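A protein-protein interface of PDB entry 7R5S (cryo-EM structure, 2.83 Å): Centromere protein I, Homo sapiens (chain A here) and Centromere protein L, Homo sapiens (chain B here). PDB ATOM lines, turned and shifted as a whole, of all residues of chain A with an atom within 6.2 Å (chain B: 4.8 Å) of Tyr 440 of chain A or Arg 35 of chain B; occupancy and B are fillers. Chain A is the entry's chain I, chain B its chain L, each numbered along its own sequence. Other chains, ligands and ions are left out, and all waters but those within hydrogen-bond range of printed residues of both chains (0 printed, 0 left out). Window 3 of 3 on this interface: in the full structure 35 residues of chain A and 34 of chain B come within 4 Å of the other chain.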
ATOM      1  N   TYR A 389      -1.536  31.427  14.215  1.00  0.00           N
ATOM      2  CA  TYR A 389      -0.594  30.864  13.256  1.00  0.00           C
ATOM      3  C   TYR A 389      -0.971  29.435  12.897  1.00  0.00           C
ATOM      4  O   TYR A 389      -1.022  29.076  11.717  1.00  0.00           O
ATOM      5  CB  TYR A 389       0.828  30.919  13.819  1.00  0.00           C
ATOM      6  CG  TYR A 389       1.823  30.078  13.050  1.00  0.00           C
ATOM      7  CD1 TYR A 389       2.437  30.568  11.906  1.00  0.00           C
ATOM      8  CD2 TYR A 389       2.147  28.794  13.467  1.00  0.00           C
ATOM      9  CE1 TYR A 389       3.343  29.804  11.198  1.00  0.00           C
ATOM     10  CE2 TYR A 389       3.051  28.021  12.764  1.00  0.00           C
ATOM     11  CZ  TYR A 389       3.647  28.532  11.632  1.00  0.00           C
ATOM     12  OH  TYR A 389       4.549  27.767  10.932  1.00  0.00           O
ATOM     13  N   CYS A 435       1.285  33.236   6.263  1.00  0.00           N
ATOM     14  CA  CYS A 435       1.331  33.569   4.844  1.00  0.00           C
ATOM     15  C   CYS A 435       2.747  33.448   4.296  1.00  0.00           C
ATOM     16  O   CYS A 435       2.943  32.970   3.174  1.00  0.00           O
ATOM     17  CB  CYS A 435       0.784  34.977   4.618  1.00  0.00           C
ATOM     18  SG  CYS A 435      -0.953  35.180   5.074  1.00  0.00           S
ATOM     19  N   GLU A 436       3.746  33.862   5.078  1.00  0.00           N
ATOM     20  CA  GLU A 436       5.133  33.733   4.638  1.00  0.00           C
ATOM     21  C   GLU A 436       5.535  32.270   4.500  1.00  0.00           C
ATOM     22  O   GLU A 436       6.204  31.891   3.529  1.00  0.00           O
ATOM     23  CB  GLU A 436       6.058  34.457   5.617  1.00  0.00           C
ATOM     24  CG  GLU A 436       7.522  34.431   5.226  1.00  0.00           C
ATOM     25  CD  GLU A 436       8.407  35.126   6.240  1.00  0.00           C
ATOM     26  OE1 GLU A 436       7.874  35.610   7.262  1.00  0.00           O
ATOM     27  OE2 GLU A 436       9.634  35.190   6.020  1.00  0.00           O
ATOM     28  N   ALA A 437       5.135  31.431   5.460  1.00  0.00           N
ATOM     29  CA  ALA A 437       5.433  30.006   5.363  1.00  0.00           C
ATOM     30  C   ALA A 437       4.745  29.378   4.156  1.00  0.00           C
ATOM     31  O   ALA A 437       5.347  28.569   3.439  1.00  0.00           O
ATOM     32  CB  ALA A 437       5.019  29.294   6.650  1.00  0.00           C
ATOM     33  N   PHE A 438       3.483  29.742   3.914  1.00  0.00           N
ATOM     34  CA  PHE A 438       2.769  29.214   2.756  1.00  0.00           C
ATOM     35  C   PHE A 438       3.424  29.656   1.454  1.00  0.00           C
ATOM     36  O   PHE A 438       3.504  28.881   0.495  1.00  0.00           O
ATOM     37  CB  PHE A 438       1.305  29.653   2.804  1.00  0.00           C
ATOM     38  CG  PHE A 438       0.520  29.285   1.579  1.00  0.00           C
ATOM     39  CD1 PHE A 438       0.128  27.976   1.360  1.00  0.00           C
ATOM     40  CD2 PHE A 438       0.166  30.249   0.651  1.00  0.00           C
ATOM     41  CE1 PHE A 438      -0.597  27.634   0.236  1.00  0.00           C
ATOM     42  CE2 PHE A 438      -0.559  29.913  -0.475  1.00  0.00           C
ATOM     43  CZ  PHE A 438      -0.942  28.605  -0.682  1.00  0.00           C
ATOM     44  N   LEU A 439       3.899  30.904   1.401  1.00  0.00           N
ATOM     45  CA  LEU A 439       4.608  31.380   0.218  1.00  0.00           C
ATOM     46  C   LEU A 439       5.897  30.601  -0.001  1.00  0.00           C
ATOM     47  O   LEU A 439       6.202  30.202  -1.130  1.00  0.00           O
ATOM     48  CB  LEU A 439       4.904  32.873   0.345  1.00  0.00           C
ATOM     49  CG  LEU A 439       3.740  33.838   0.127  1.00  0.00           C
ATOM     50  CD1 LEU A 439       4.124  35.240   0.568  1.00  0.00           C
ATOM     51  CD2 LEU A 439       3.308  33.834  -1.328  1.00  0.00           C
ATOM     52  N   TYR A 440       6.666  30.373   1.066  1.00  0.00           N
ATOM     53  CA  TYR A 440       7.905  29.614   0.927  1.00  0.00           C
ATOM     54  C   TYR A 440       7.638  28.170   0.522  1.00  0.00           C
ATOM     55  O   TYR A 440       8.465  27.556  -0.163  1.00  0.00           O
ATOM     56  CB  TYR A 440       8.703  29.655   2.230  1.00  0.00           C
ATOM     57  CG  TYR A 440       9.303  31.004   2.552  1.00  0.00           C
ATOM     58  CD1 TYR A 440       9.408  31.991   1.582  1.00  0.00           C
ATOM     59  CD2 TYR A 440       9.770  31.288   3.828  1.00  0.00           C
ATOM     60  CE1 TYR A 440       9.957  33.224   1.874  1.00  0.00           C
ATOM     61  CE2 TYR A 440      10.320  32.517   4.129  1.00  0.00           C
ATOM     62  CZ  TYR A 440      10.412  33.481   3.149  1.00  0.00           C
ATOM     63  OH  TYR A 440      10.959  34.707   3.446  1.00  0.00           O
ATOM     64  N   LYS A 441       6.498  27.612   0.931  1.00  0.00           N
ATOM     65  CA  LYS A 441       6.213  26.212   0.633  1.00  0.00           C
ATOM     66  C   LYS A 441       5.681  26.025  -0.784  1.00  0.00           C
ATOM     67  O   LYS A 441       6.142  25.141  -1.515  1.00  0.00           O
ATOM     68  CB  LYS A 441       5.213  25.652   1.647  1.00  0.00           C
ATOM     69  CG  LYS A 441       5.802  25.349   3.012  1.00  0.00           C
ATOM     70  CD  LYS A 441       4.748  24.771   3.939  1.00  0.00           C
ATOM     71  CE  LYS A 441       5.330  24.424   5.297  1.00  0.00           C
ATOM     72  NZ  LYS A 441       4.304  23.857   6.213  1.00  0.00           N
ATOM     73  N   SER A 442       4.711  26.842  -1.192  1.00  0.00           N
ATOM     74  CA  SER A 442       3.963  26.605  -2.421  1.00  0.00           C
ATOM     75  C   SER A 442       4.490  27.379  -3.623  1.00  0.00           C
ATOM     76  O   SER A 442       3.883  27.309  -4.695  1.00  0.00           O
ATOM     77  CB  SER A 442       2.485  26.947  -2.205  1.00  0.00           C
ATOM     78  OG  SER A 442       2.332  28.285  -1.769  1.00  0.00           O
ATOM     79  N   LEU A 443       5.592  28.107  -3.480  1.00  0.00           N
ATOM     80  CA  LEU A 443       6.117  28.892  -4.594  1.00  0.00           C
ATOM     81  C   LEU A 443       6.740  28.024  -5.688  1.00  0.00           C
ATOM     82  O   LEU A 443       6.470  28.265  -6.871  1.00  0.00           O
ATOM     83  CB  LEU A 443       7.134  29.921  -4.095  1.00  0.00           C
ATOM     84  CG  LEU A 443       7.605  30.941  -5.131  1.00  0.00           C
ATOM     85  CD1 LEU A 443       6.450  31.819  -5.583  1.00  0.00           C
ATOM     86  CD2 LEU A 443       8.733  31.785  -4.571  1.00  0.00           C
ATOM     87  N   PRO A 444       7.579  27.028  -5.366  1.00  0.00           N
ATOM     88  CA  PRO A 444       8.173  26.216  -6.443  1.00  0.00           C
ATOM     89  C   PRO A 444       7.161  25.452  -7.278  1.00  0.00           C
ATOM     90  O   PRO A 444       7.485  25.063  -8.407  1.00  0.00           O
ATOM     91  CB  PRO A 444       9.107  25.259  -5.688  1.00  0.00           C
ATOM     92  CG  PRO A 444       9.415  25.957  -4.424  1.00  0.00           C
ATOM     93  CD  PRO A 444       8.152  26.665  -4.057  1.00  0.00           C
ATOM     94  N   ILE A 462       5.929  41.040   3.093  1.00  0.00           N
ATOM     95  CA  ILE A 462       7.003  40.192   3.609  1.00  0.00           C
ATOM     96  C   ILE A 462       7.809  41.010   4.609  1.00  0.00           C
ATOM     97  O   ILE A 462       8.184  42.147   4.300  1.00  0.00           O
ATOM     98  CB  ILE A 462       7.911  39.665   2.479  1.00  0.00           C
ATOM     99  CG1 ILE A 462       7.223  38.524   1.729  1.00  0.00           C
ATOM    100  CG2 ILE A 462       9.250  39.202   3.031  1.00  0.00           C
ATOM    101  CD1 ILE A 462       6.937  37.314   2.587  1.00  0.00           C
ATOM    102  N   SER A 465      14.025  41.662   6.014  1.00  0.00           N
ATOM    103  CA  SER A 465      15.104  40.738   6.328  1.00  0.00           C
ATOM    104  C   SER A 465      16.254  40.990   5.365  1.00  0.00           C
ATOM    105  O   SER A 465      16.149  41.790   4.432  1.00  0.00           O
ATOM    106  CB  SER A 465      14.635  39.282   6.253  1.00  0.00           C
ATOM    107  OG  SER A 465      14.353  38.904   4.916  1.00  0.00           O
ATOM    108  N   VAL A 470      16.811  35.876   2.071  1.00  0.00           N
ATOM    109  CA  VAL A 470      15.501  35.756   1.435  1.00  0.00           C
ATOM    110  C   VAL A 470      15.592  35.554  -0.071  1.00  0.00           C
ATOM    111  O   VAL A 470      14.569  35.262  -0.711  1.00  0.00           O
ATOM    112  CB  VAL A 470      14.642  36.998   1.750  1.00  0.00           C
ATOM    113  CG1 VAL A 470      14.978  38.141   0.802  1.00  0.00           C
ATOM    114  CG2 VAL A 470      13.156  36.658   1.701  1.00  0.00           C
ATOM    115  N   LEU A 473      15.000  31.662  -1.367  1.00  0.00           N
ATOM    116  CA  LEU A 473      13.689  31.102  -1.062  1.00  0.00           C
ATOM    117  C   LEU A 473      12.608  31.655  -1.982  1.00  0.00           C
ATOM    118  O   LEU A 473      11.686  30.928  -2.366  1.00  0.00           O
ATOM    119  CB  LEU A 473      13.333  31.375   0.400  1.00  0.00           C
ATOM    120  CG  LEU A 473      14.239  30.735   1.452  1.00  0.00           C
ATOM    121  CD1 LEU A 473      13.833  31.175   2.848  1.00  0.00           C
ATOM    122  CD2 LEU A 473      14.205  29.220   1.336  1.00  0.00           C
ATOM    123  N   LEU A 474      12.701  32.933  -2.343  1.00  0.00           N
ATOM    124  CA  LEU A 474      11.660  33.604  -3.112  1.00  0.00           C
ATOM    125  C   LEU A 474      12.142  34.100  -4.466  1.00  0.00           C
ATOM    126  O   LEU A 474      11.513  33.802  -5.492  1.00  0.00           O
ATOM    127  CB  LEU A 474      11.096  34.781  -2.298  1.00  0.00           C
ATOM    128  CG  LEU A 474       9.955  35.592  -2.914  1.00  0.00           C
ATOM    129  CD1 LEU A 474       8.620  34.902  -2.697  1.00  0.00           C
ATOM    130  CD2 LEU A 474       9.935  37.002  -2.344  1.00  0.00           C
ATOM    131  N   LEU B  31      10.358  28.917  15.836  1.00  0.00           N
ATOM    132  CA  LEU B  31       9.428  28.184  14.987  1.00  0.00           C
ATOM    133  C   LEU B  31       9.608  28.566  13.523  1.00  0.00           C
ATOM    134  O   LEU B  31       9.652  27.699  12.643  1.00  0.00           O
ATOM    135  CB  LEU B  31       7.992  28.442  15.444  1.00  0.00           C
ATOM    136  CG  LEU B  31       6.868  27.825  14.611  1.00  0.00           C
ATOM    137  CD1 LEU B  31       7.057  26.322  14.467  1.00  0.00           C
ATOM    138  CD2 LEU B  31       5.524  28.137  15.243  1.00  0.00           C
ATOM    139  N   GLU B  32       9.725  29.866  13.245  1.00  0.00           N
ATOM    140  CA  GLU B  32       9.943  30.303  11.868  1.00  0.00           C
ATOM    141  C   GLU B  32      11.280  29.801  11.336  1.00  0.00           C
ATOM    142  O   GLU B  32      11.396  29.446  10.156  1.00  0.00           O
ATOM    143  CB  GLU B  32       9.865  31.826  11.781  1.00  0.00           C
ATOM    144  CG  GLU B  32       9.778  32.362  10.362  1.00  0.00           C
ATOM    145  CD  GLU B  32       8.468  32.011   9.682  1.00  0.00           C
ATOM    146  OE1 GLU B  32       7.463  31.802  10.394  1.00  0.00           O
ATOM    147  OE2 GLU B  32       8.443  31.944   8.436  1.00  0.00           O
ATOM    148  N   SER B  33      12.301  29.756  12.196  1.00  0.00           N
ATOM    149  CA  SER B  33      13.615  29.286  11.771  1.00  0.00           C
ATOM    150  C   SER B  33      13.583  27.805  11.417  1.00  0.00           C
ATOM    151  O   SER B  33      14.115  27.394  10.380  1.00  0.00           O
ATOM    152  CB  SER B  33      14.646  29.558  12.867  1.00  0.00           C
ATOM    153  OG  SER B  33      15.965  29.501  12.353  1.00  0.00           O
ATOM    154  N   VAL B  34      12.961  26.983  12.268  1.00  0.00           N
ATOM    155  CA  VAL B  34      12.895  25.555  11.974  1.00  0.00           C
ATOM    156  C   VAL B  34      11.947  25.296  10.807  1.00  0.00           C
ATOM    157  O   VAL B  34      12.071  24.283  10.108  1.00  0.00           O
ATOM    158  CB  VAL B  34      12.494  24.756  13.231  1.00  0.00           C
ATOM    159  CG1 VAL B  34      11.121  25.170  13.728  1.00  0.00           C
ATOM    160  CG2 VAL B  34      12.553  23.255  12.973  1.00  0.00           C
ATOM    161  N   ARG B  35      11.006  26.209  10.556  1.00  0.00           N
ATOM    162  CA  ARG B  35      10.126  26.067   9.403  1.00  0.00           C
ATOM    163  C   ARG B  35      10.882  26.323   8.103  1.00  0.00           C
ATOM    164  O   ARG B  35      10.881  25.485   7.194  1.00  0.00           O
ATOM    165  CB  ARG B  35       8.934  27.019   9.537  1.00  0.00           C
ATOM    166  CG  ARG B  35       7.590  26.406   9.168  1.00  0.00           C
ATOM    167  CD  ARG B  35       7.559  25.978   7.713  1.00  0.00           C
ATOM    168  NE  ARG B  35       8.113  27.007   6.838  1.00  0.00           N
ATOM    169  CZ  ARG B  35       8.539  26.784   5.600  1.00  0.00           C
ATOM    170  NH1 ARG B  35       8.479  25.565   5.082  1.00  0.00           N
ATOM    171  NH2 ARG B  35       9.030  27.783   4.879  1.00  0.00           N
ATOM    172  N   LYS B  36      11.536  27.482   7.998  1.00  0.00           N
ATOM    173  CA  LYS B  36      12.248  27.824   6.770  1.00  0.00           C
ATOM    174  C   LYS B  36      13.510  26.998   6.563  1.00  0.00           C
ATOM    175  O   LYS B  36      14.127  27.101   5.498  1.00  0.00           O
ATOM    176  CB  LYS B  36      12.599  29.313   6.761  1.00  0.00           C
ATOM    177  CG  LYS B  36      13.662  29.713   7.770  1.00  0.00           C
ATOM    178  CD  LYS B  36      14.021  31.183   7.632  1.00  0.00           C
ATOM    179  CE  LYS B  36      12.804  32.070   7.846  1.00  0.00           C
ATOM    180  NZ  LYS B  36      13.136  33.514   7.711  1.00  0.00           N
ATOM    181  N   GLN B  37      13.907  26.187   7.545  1.00  0.00           N
ATOM    182  CA  GLN B  37      15.089  25.347   7.404  1.00  0.00           C
ATOM    183  C   GLN B  37      14.809  24.064   6.632  1.00  0.00           C
ATOM    184  O   GLN B  37      15.752  23.430   6.144  1.00  0.00           O
ATOM    185  CB  GLN B  37      15.654  25.009   8.788  1.00  0.00           C
ATOM    186  CG  GLN B  37      17.079  24.479   8.784  1.00  0.00           C
ATOM    187  CD  GLN B  37      17.135  22.967   8.870  1.00  0.00           C
ATOM    188  OE1 GLN B  37      16.103  22.298   8.927  1.00  0.00           O
ATOM    189  NE2 GLN B  37      18.345  22.419   8.882  1.00  0.00           N
ATOM    190  N   SER B  38      13.541  23.674   6.497  1.00  0.00           N
ATOM    191  CA  SER B  38      13.171  22.432   5.818  1.00  0.00           C
ATOM    192  C   SER B  38      13.261  22.648   4.309  1.00  0.00           C
ATOM    193  O   SER B  38      12.277  22.937   3.623  1.00  0.00           O
ATOM    194  CB  SER B  38      11.779  21.983   6.240  1.00  0.00           C
ATOM    195  OG  SER B  38      11.214  21.108   5.279  1.00  0.00           O
ATOM    196  N   GLU B 344       4.084  20.670  10.597  1.00  0.00           N
ATOM    197  CA  GLU B 344       5.108  21.710  10.562  1.00  0.00           C
ATOM    198  C   GLU B 344       5.846  21.716   9.229  1.00  0.00           C
ATOM    199  O   GLU B 344       5.388  21.134   8.246  1.00  0.00           O
ATOM    200  CB  GLU B 344       6.103  21.524  11.710  1.00  0.00           C
ATOM    201  CG  GLU B 344       5.647  22.122  13.030  1.00  0.00           C
ATOM    202  CD  GLU B 344       6.781  22.260  14.026  1.00  0.00           C
ATOM    203  OE1 GLU B 344       7.815  21.582  13.848  1.00  0.00           O
ATOM    204  OE2 GLU B 344       6.642  23.051  14.981  1.00  0.00           O
ATOM    205  OXT GLU B 344       6.916  22.309   9.102  1.00  0.00           O
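O of Glu 344 of chain B lies within salt-bridge range of NZ of Lys 441 of chain A (3.6 Å).
The side-chain carboxylate (OE2) of Glu 436 of chain A lies within hydrogen-bond range of the side-chain hydroxyl (OH) of Tyr 440 of chain A (2.9 Å).
Tyr 389 of chain A touches Leu 31 of chain B. OH of Tyr 389 of chain A touches CG of Arg 35 of chain B, 3.8 Å away. Glu 436 of chain A touches Glu 32 of chain B. Ala 437 of chain A touches Arg 35 of chain B (CB to NE, 3.9 Å). Tyr 440 of chain A touches Arg 35 of chain B (CB to NH2, 3.3 Å). CE of Lys 441 of chain A touches NH1 of Arg 35 of chain B (3.4 Å).
Of chain B, only Arg 35 comes within 4 Å of Tyr 440 of chain A. Arg 35 of chain B touches four residues of chain A. Printed residues of chain A within 4 Å of Glu 344 of chain B: Lys 441 (3.6 Å). Of the printed residues of chain B, Glu 436 of chain A touches Glu 32. Of the printed residues of chain B, Ala 437 of chain A touches Arg 35 (3.9 Å). Of the printed residues of chain A, Leu 31 of chain B touches Tyr 389 (3.5 Å). The nearest residue of chain B that does not touch Tyr 440 of chain A is Lys 36 of chain B (4.5 Å). The nearest residue of chain A that does not touch Arg 35 of chain B is Glu 436 of chain A (5.2 Å).
Of the 16 printed residues of chain A, 5 touch a printed residue of chain B. Hydrophobic or aromatic side chains of chain A within 4 Å of the printed part of chain B: Tyr 389, Ala 437 and Tyr 440. Hydrophobic or aromatic side chains of chain B that line the printed part of chain A: Leu 31.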
